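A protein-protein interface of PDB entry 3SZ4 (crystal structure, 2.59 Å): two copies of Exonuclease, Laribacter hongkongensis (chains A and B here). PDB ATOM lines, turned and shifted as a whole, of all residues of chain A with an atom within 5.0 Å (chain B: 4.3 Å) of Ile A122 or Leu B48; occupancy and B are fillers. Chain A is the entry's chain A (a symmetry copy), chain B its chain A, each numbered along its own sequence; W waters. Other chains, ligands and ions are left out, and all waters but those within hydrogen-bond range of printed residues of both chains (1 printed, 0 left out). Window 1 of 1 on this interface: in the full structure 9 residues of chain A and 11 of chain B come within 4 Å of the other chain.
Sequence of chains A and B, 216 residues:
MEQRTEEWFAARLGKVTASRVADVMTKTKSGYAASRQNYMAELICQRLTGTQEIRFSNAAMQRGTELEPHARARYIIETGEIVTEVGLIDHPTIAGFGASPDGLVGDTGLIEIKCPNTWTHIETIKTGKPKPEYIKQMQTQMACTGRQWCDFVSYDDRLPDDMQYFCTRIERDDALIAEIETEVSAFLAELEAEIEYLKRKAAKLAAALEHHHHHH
Cys B45 touches Thr A118.
Thr A118 touches Thr B49 (CG2 to CG2, 3.7 Å).
Cys B45 touches Trp A119 (SG to N, 3.9 Å).
Ile A122 touches Leu B48 (CD1 to CD1, 3.8 Å).
CG2 of Ile A122 touches CD2 of Leu B198, 3.7 Å away.
CD1 of Leu B198 touches CD of Lys A126, at 3.9 Å.
Arg A158 touches Thr B49.
Leu A159 touches Leu B48 (CD2 to CB, 3.9 Å).
Leu A159 touches Thr B49.
Met A163 touches Leu B48 (CE to CD2, 3.8 Å).
Water W1 bridges O of Thr B49 (3.0 Å) and O of Arg A158 (3.0 Å).
No position is printed for both chains.
Of the 11 pairs that touch across the chains among the printed residues, none has its exchanged pair printed and touching as well.
Of chain B, only Leu B48 and Leu B198 come within 4 Å of Ile A122.
Leu B48 touches just these residues of chain A: Ile A122 (3.8 Å), Leu A159 (3.9 Å), Pro A160 (3.2 Å) and Met A163 (3.8 Å).
Of the printed residues of chain B, Leu A159 touches Leu B48 (3.9 Å) and Thr B49 (3.9 Å).
Of the printed residues of chain A, Leu B198 touches Ile A122 (3.7 Å) and Lys A126 (3.9 Å).
Of the printed residues of chain B, Trp A119 touches Cys B45 (3.9 Å).
Of the printed residues of chain B, Pro A160 touches Leu B48.
Of the printed residues of chain B, Thr A118 touches Cys B45 (3.8 Å) and Thr B49 (3.7 Å).
Gly B50 touches none of the printed residues of chain A.
Thr A124 touches none of the printed residues of chain B.
The nearest printed residue of chain B that does not touch Ile A122 is Cys B45 (4.4 Å).
The nearest printed residue of chain B that does not touch Lys A126 is Ile B44 (6.4 Å).
The backbone carbonyl oxygen of Cys B45 lies within hydrogen-bond range of the side-chain hydroxyl of Thr B49, 2.6 Å away.
OG1 of Thr A118 sits close to NE of Arg A158 (3.4 Å).
OE2 of Glu A123 sits at hydrogen-bond distance from NE1 of Trp A119.
O of Met A163 lies close to ND1 of His A121 (3.3 Å).
Of the 8 printed residues of chain B, 4 touch a printed residue of chain A.
Hydrophobic or aromatic side chains of chain B within 4 Å of the printed part of chain A: Leu B48 and Leu B198.
Along chain B the printed residues that touch a printed residue of chain A span positions 45 to 198.
Printed residues of chain A that touch a printed residue of chain B: Thr A118, Trp A119, Ile A122, Lys A126, Arg A158, Leu A159, Pro A160 and Met A163.
Among the printed residues, 11 pairs touch across the chains.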
ATOM      1  N   THR A 118     -27.278   8.955  -2.765  1.00  0.00           N
ATOM      2  CA  THR A 118     -26.346   8.279  -3.630  1.00  0.00           C
ATOM      3  C   THR A 118     -24.876   8.474  -3.242  1.00  0.00           C
ATOM      4  O   THR A 118     -24.077   7.513  -3.273  1.00  0.00           O
ATOM      5  CB  THR A 118     -26.558   8.723  -5.052  1.00  0.00           C
ATOM      6  OG1 THR A 118     -27.961   8.767  -5.324  1.00  0.00           O
ATOM      7  CG2 THR A 118     -25.902   7.755  -5.975  1.00  0.00           C
ATOM      8  N   TRP A 119     -24.504   9.696  -2.872  1.00  0.00           N
ATOM      9  CA  TRP A 119     -23.096   9.964  -2.567  1.00  0.00           C
ATOM     10  C   TRP A 119     -22.599   9.274  -1.290  1.00  0.00           C
ATOM     11  O   TRP A 119     -21.458   8.822  -1.215  1.00  0.00           O
ATOM     12  CB  TRP A 119     -22.774  11.457  -2.520  1.00  0.00           C
ATOM     13  CG  TRP A 119     -21.325  11.630  -2.223  1.00  0.00           C
ATOM     14  CD1 TRP A 119     -20.772  12.114  -1.066  1.00  0.00           C
ATOM     15  CD2 TRP A 119     -20.224  11.240  -3.063  1.00  0.00           C
ATOM     16  NE1 TRP A 119     -19.401  12.081  -1.150  1.00  0.00           N
ATOM     17  CE2 TRP A 119     -19.037  11.556  -2.365  1.00  0.00           C
ATOM     18  CE3 TRP A 119     -20.130  10.674  -4.346  1.00  0.00           C
ATOM     19  CZ2 TRP A 119     -17.762  11.318  -2.903  1.00  0.00           C
ATOM     20  CZ3 TRP A 119     -18.863  10.434  -4.886  1.00  0.00           C
ATOM     21  CH2 TRP A 119     -17.694  10.761  -4.160  1.00  0.00           C
ATOM     22  N   THR A 120     -23.463   9.222  -0.286  1.00  0.00           N
ATOM     23  CA  THR A 120     -23.166   8.517   0.929  1.00  0.00           C
ATOM     24  C   THR A 120     -23.027   7.047   0.594  1.00  0.00           C
ATOM     25  O   THR A 120     -22.170   6.374   1.138  1.00  0.00           O
ATOM     26  CB  THR A 120     -24.322   8.660   1.906  1.00  0.00           C
ATOM     27  OG1 THR A 120     -24.703  10.042   2.001  1.00  0.00           O
ATOM     28  CG2 THR A 120     -23.972   8.076   3.269  1.00  0.00           C
ATOM     29  N   HIS A 121     -23.856   6.535  -0.302  1.00  0.00           N
ATOM     30  CA  HIS A 121     -23.792   5.115  -0.614  1.00  0.00           C
ATOM     31  C   HIS A 121     -22.465   4.805  -1.254  1.00  0.00           C
ATOM     32  O   HIS A 121     -21.787   3.852  -0.852  1.00  0.00           O
ATOM     33  CB  HIS A 121     -24.925   4.668  -1.542  1.00  0.00           C
ATOM     34  CG  HIS A 121     -24.983   3.183  -1.744  1.00  0.00           C
ATOM     35  ND1 HIS A 121     -24.753   2.584  -2.966  1.00  0.00           N
ATOM     36  CD2 HIS A 121     -25.236   2.175  -0.878  1.00  0.00           C
ATOM     37  CE1 HIS A 121     -24.867   1.275  -2.842  1.00  0.00           C
ATOM     38  NE2 HIS A 121     -25.165   1.000  -1.587  1.00  0.00           N
ATOM     39  N   ILE A 122     -22.101   5.606  -2.249  1.00  0.00           N
ATOM     40  CA  ILE A 122     -20.847   5.437  -2.960  1.00  0.00           C
ATOM     41  C   ILE A 122     -19.654   5.461  -2.031  1.00  0.00           C
ATOM     42  O   ILE A 122     -18.712   4.686  -2.224  1.00  0.00           O
ATOM     43  CB  ILE A 122     -20.649   6.519  -4.000  1.00  0.00           C
ATOM     44  CG1 ILE A 122     -21.615   6.278  -5.164  1.00  0.00           C
ATOM     45  CG2 ILE A 122     -19.187   6.547  -4.456  1.00  0.00           C
ATOM     46  CD1 ILE A 122     -21.678   7.415  -6.194  1.00  0.00           C
ATOM     47  N   GLU A 123     -19.677   6.328  -1.020  1.00  0.00           N
ATOM     48  CA  GLU A 123     -18.556   6.350  -0.086  1.00  0.00           C
ATOM     49  C   GLU A 123     -18.459   5.094   0.774  1.00  0.00           C
ATOM     50  O   GLU A 123     -17.381   4.743   1.230  1.00  0.00           O
ATOM     51  CB  GLU A 123     -18.504   7.638   0.738  1.00  0.00           C
ATOM     52  CG  GLU A 123     -17.652   8.702   0.045  1.00  0.00           C
ATOM     53  CD  GLU A 123     -17.482   9.980   0.866  1.00  0.00           C
ATOM     54  OE1 GLU A 123     -18.124  10.123   1.934  1.00  0.00           O
ATOM     55  OE2 GLU A 123     -16.695  10.855   0.437  1.00  0.00           O
ATOM     56  N   THR A 124     -19.582   4.426   0.986  1.00  0.00           N
ATOM     57  CA  THR A 124     -19.578   3.110   1.603  1.00  0.00           C
ATOM     58  C   THR A 124     -18.996   2.017   0.709  1.00  0.00           C
ATOM     59  O   THR A 124     -18.248   1.136   1.175  1.00  0.00           O
ATOM     60  CB  THR A 124     -20.973   2.730   1.962  1.00  0.00           C
ATOM     61  OG1 THR A 124     -21.330   3.499   3.091  1.00  0.00           O
ATOM     62  CG2 THR A 124     -21.057   1.285   2.332  1.00  0.00           C
ATOM     63  N   ILE A 125     -19.372   2.042  -0.569  1.00  0.00           N
ATOM     64  CA  ILE A 125     -18.725   1.155  -1.504  1.00  0.00           C
ATOM     65  C   ILE A 125     -17.226   1.480  -1.505  1.00  0.00           C
ATOM     66  O   ILE A 125     -16.387   0.579  -1.439  1.00  0.00           O
ATOM     67  CB  ILE A 125     -19.256   1.308  -2.913  1.00  0.00           C
ATOM     68  CG1 ILE A 125     -20.648   0.679  -3.032  1.00  0.00           C
ATOM     69  CG2 ILE A 125     -18.276   0.651  -3.876  1.00  0.00           C
ATOM     70  CD1 ILE A 125     -21.370   1.070  -4.262  1.00  0.00           C
ATOM     71  N   LYS A 126     -16.902   2.769  -1.552  1.00  0.00           N
ATOM     72  CA  LYS A 126     -15.515   3.170  -1.664  1.00  0.00           C
ATOM     73  C   LYS A 126     -14.665   2.629  -0.520  1.00  0.00           C
ATOM     74  O   LYS A 126     -13.627   2.025  -0.789  1.00  0.00           O
ATOM     75  CB  LYS A 126     -15.366   4.672  -1.827  1.00  0.00           C
ATOM     76  CG  LYS A 126     -15.445   5.128  -3.288  1.00  0.00           C
ATOM     77  CD  LYS A 126     -14.681   6.469  -3.538  1.00  0.00           C
ATOM     78  CE  LYS A 126     -15.045   7.557  -2.513  1.00  0.00           C
ATOM     79  NZ  LYS A 126     -14.908   8.969  -3.022  1.00  0.00           N
ATOM     80  N   ARG A 158     -30.803   3.864  -7.592  1.00  0.00           N
ATOM     81  CA  ARG A 158     -30.633   4.813  -8.685  1.00  0.00           C
ATOM     82  C   ARG A 158     -29.345   4.546  -9.484  1.00  0.00           C
ATOM     83  O   ARG A 158     -29.101   5.156 -10.534  1.00  0.00           O
ATOM     84  CB  ARG A 158     -30.669   6.241  -8.157  1.00  0.00           C
ATOM     85  CG  ARG A 158     -31.990   6.622  -7.478  1.00  0.00           C
ATOM     86  CD  ARG A 158     -31.789   7.778  -6.499  1.00  0.00           C
ATOM     87  NE  ARG A 158     -31.096   7.379  -5.265  1.00  0.00           N
ATOM     88  CZ  ARG A 158     -31.059   8.113  -4.150  1.00  0.00           C
ATOM     89  NH1 ARG A 158     -31.689   9.274  -4.120  1.00  0.00           N
ATOM     90  NH2 ARG A 158     -30.403   7.701  -3.065  1.00  0.00           N
ATOM     91  N   LEU A 159     -28.543   3.611  -8.990  1.00  0.00           N
ATOM     92  CA  LEU A 159     -27.210   3.350  -9.512  1.00  0.00           C
ATOM     93  C   LEU A 159     -27.210   2.213 -10.513  1.00  0.00           C
ATOM     94  O   LEU A 159     -28.141   1.417 -10.549  1.00  0.00           O
ATOM     95  CB  LEU A 159     -26.256   3.015  -8.362  1.00  0.00           C
ATOM     96  CG  LEU A 159     -25.901   4.235  -7.528  1.00  0.00           C
ATOM     97  CD1 LEU A 159     -25.131   3.849  -6.265  1.00  0.00           C
ATOM     98  CD2 LEU A 159     -25.119   5.275  -8.331  1.00  0.00           C
ATOM     99  N   PRO A 160     -26.152   2.135 -11.330  1.00  0.00           N
ATOM    100  CA  PRO A 160     -25.927   0.936 -12.125  1.00  0.00           C
ATOM    101  C   PRO A 160     -26.010  -0.272 -11.221  1.00  0.00           C
ATOM    102  O   PRO A 160     -25.795  -0.157  -9.994  1.00  0.00           O
ATOM    103  CB  PRO A 160     -24.506   1.116 -12.606  1.00  0.00           C
ATOM    104  CG  PRO A 160     -24.369   2.589 -12.732  1.00  0.00           C
ATOM    105  CD  PRO A 160     -25.115   3.150 -11.570  1.00  0.00           C
ATOM    106  N   MET A 163     -23.674  -1.485  -8.429  1.00  0.00           N
ATOM    107  CA  MET A 163     -23.330  -0.534  -7.390  1.00  0.00           C
ATOM    108  C   MET A 163     -24.483  -0.337  -6.440  1.00  0.00           C
ATOM    109  O   MET A 163     -24.360   0.389  -5.453  1.00  0.00           O
ATOM    110  CB  MET A 163     -22.986   0.795  -8.011  1.00  0.00           C
ATOM    111  CG  MET A 163     -21.836   0.720  -8.949  1.00  0.00           C
ATOM    112  SD  MET A 163     -21.337   2.374  -9.390  1.00  0.00           S
ATOM    113  CE  MET A 163     -20.349   2.027 -10.856  1.00  0.00           C
ATOM    114  N   ILE B  44     -20.674  13.346 -10.246  1.00  0.00           N
ATOM    115  CA  ILE B  44     -20.515  11.901 -10.269  1.00  0.00           C
ATOM    116  C   ILE B  44     -21.885  11.203 -10.211  1.00  0.00           C
ATOM    117  O   ILE B  44     -22.219  10.418 -11.111  1.00  0.00           O
ATOM    118  CB  ILE B  44     -19.627  11.434  -9.140  1.00  0.00           C
ATOM    119  CG1 ILE B  44     -18.322  12.245  -9.177  1.00  0.00           C
ATOM    120  CG2 ILE B  44     -19.448   9.903  -9.220  1.00  0.00           C
ATOM    121  CD1 ILE B  44     -17.205  11.687  -8.400  1.00  0.00           C
ATOM    122  N   CYS B  45     -22.687  11.525  -9.195  1.00  0.00           N
ATOM    123  CA  CYS B  45     -24.061  11.050  -9.095  1.00  0.00           C
ATOM    124  C   CYS B  45     -24.926  11.288 -10.308  1.00  0.00           C
ATOM    125  O   CYS B  45     -25.722  10.429 -10.690  1.00  0.00           O
ATOM    126  CB  CYS B  45     -24.745  11.707  -7.920  1.00  0.00           C
ATOM    127  SG  CYS B  45     -24.001  11.175  -6.425  1.00  0.00           S
ATOM    128  N   GLN B  46     -24.810  12.458 -10.911  1.00  0.00           N
ATOM    129  CA  GLN B  46     -25.631  12.729 -12.077  1.00  0.00           C
ATOM    130  C   GLN B  46     -25.298  11.768 -13.200  1.00  0.00           C
ATOM    131  O   GLN B  46     -26.209  11.246 -13.850  1.00  0.00           O
ATOM    132  CB  GLN B  46     -25.436  14.143 -12.567  1.00  0.00           C
ATOM    133  CG  GLN B  46     -26.193  15.147 -11.786  1.00  0.00           C
ATOM    134  CD  GLN B  46     -25.947  16.550 -12.276  1.00  0.00           C
ATOM    135  OE1 GLN B  46     -25.334  16.789 -13.333  1.00  0.00           O
ATOM    136  NE2 GLN B  46     -26.430  17.501 -11.511  1.00  0.00           N
ATOM    137  N   ARG B  47     -23.995  11.546 -13.413  1.00  0.00           N
ATOM    138  CA  ARG B  47     -23.514  10.638 -14.444  1.00  0.00           C
ATOM    139  C   ARG B  47     -23.884   9.212 -14.113  1.00  0.00           C
ATOM    140  O   ARG B  47     -24.392   8.503 -14.973  1.00  0.00           O
ATOM    141  CB  ARG B  47     -22.007  10.744 -14.659  1.00  0.00           C
ATOM    142  CG  ARG B  47     -21.606  11.933 -15.482  1.00  0.00           C
ATOM    143  CD  ARG B  47     -20.130  12.004 -15.662  1.00  0.00           C
ATOM    144  NE  ARG B  47     -19.687  13.333 -16.089  1.00  0.00           N
ATOM    145  CZ  ARG B  47     -18.620  13.571 -16.866  1.00  0.00           C
ATOM    146  NH1 ARG B  47     -17.879  12.569 -17.339  1.00  0.00           N
ATOM    147  NH2 ARG B  47     -18.303  14.820 -17.187  1.00  0.00           N
ATOM    148  N   LEU B  48     -23.655   8.780 -12.879  1.00  0.00           N
ATOM    149  CA  LEU B  48     -23.895   7.385 -12.556  1.00  0.00           C
ATOM    150  C   LEU B  48     -25.367   7.041 -12.469  1.00  0.00           C
ATOM    151  O   LEU B  48     -25.759   5.959 -12.867  1.00  0.00           O
ATOM    152  CB  LEU B  48     -23.204   6.990 -11.261  1.00  0.00           C
ATOM    153  CG  LEU B  48     -21.695   6.798 -11.313  1.00  0.00           C
ATOM    154  CD1 LEU B  48     -21.190   6.767  -9.900  1.00  0.00           C
ATOM    155  CD2 LEU B  48     -21.333   5.517 -12.063  1.00  0.00           C
ATOM    156  N   THR B  49     -26.183   7.945 -11.941  1.00  0.00           N
ATOM    157  CA  THR B  49     -27.602   7.632 -11.772  1.00  0.00           C
ATOM    158  C   THR B  49     -28.392   7.972 -13.027  1.00  0.00           C
ATOM    159  O   THR B  49     -29.495   7.463 -13.222  1.00  0.00           O
ATOM    160  CB  THR B  49     -28.232   8.414 -10.630  1.00  0.00           C
ATOM    161  OG1 THR B  49     -28.259   9.803 -10.995  1.00  0.00           O
ATOM    162  CG2 THR B  49     -27.465   8.190  -9.312  1.00  0.00           C
ATOM    163  N   GLY B  50     -27.844   8.844 -13.864  1.00  0.00           N
ATOM    164  CA  GLY B  50     -28.548   9.292 -15.024  1.00  0.00           C
ATOM    165  C   GLY B  50     -29.590  10.359 -14.738  1.00  0.00           C
ATOM    166  O   GLY B  50     -30.402  10.626 -15.609  1.00  0.00           O
ATOM    167  N   LEU B 198     -14.872   3.531  -9.400  1.00  0.00           N
ATOM    168  CA  LEU B 198     -15.986   2.865  -8.732  1.00  0.00           C
ATOM    169  C   LEU B 198     -16.493   1.716  -9.555  1.00  0.00           C
ATOM    170  O   LEU B 198     -16.839   0.656  -9.020  1.00  0.00           O
ATOM    171  CB  LEU B 198     -17.122   3.822  -8.551  1.00  0.00           C
ATOM    172  CG  LEU B 198     -16.966   4.876  -7.480  1.00  0.00           C
ATOM    173  CD1 LEU B 198     -15.503   5.374  -7.224  1.00  0.00           C
ATOM    174  CD2 LEU B 198     -17.877   6.031  -7.876  1.00  0.00           C
HETATM  175  O   HOH W   1     -31.673   5.856 -11.987  1.00  0.00           O
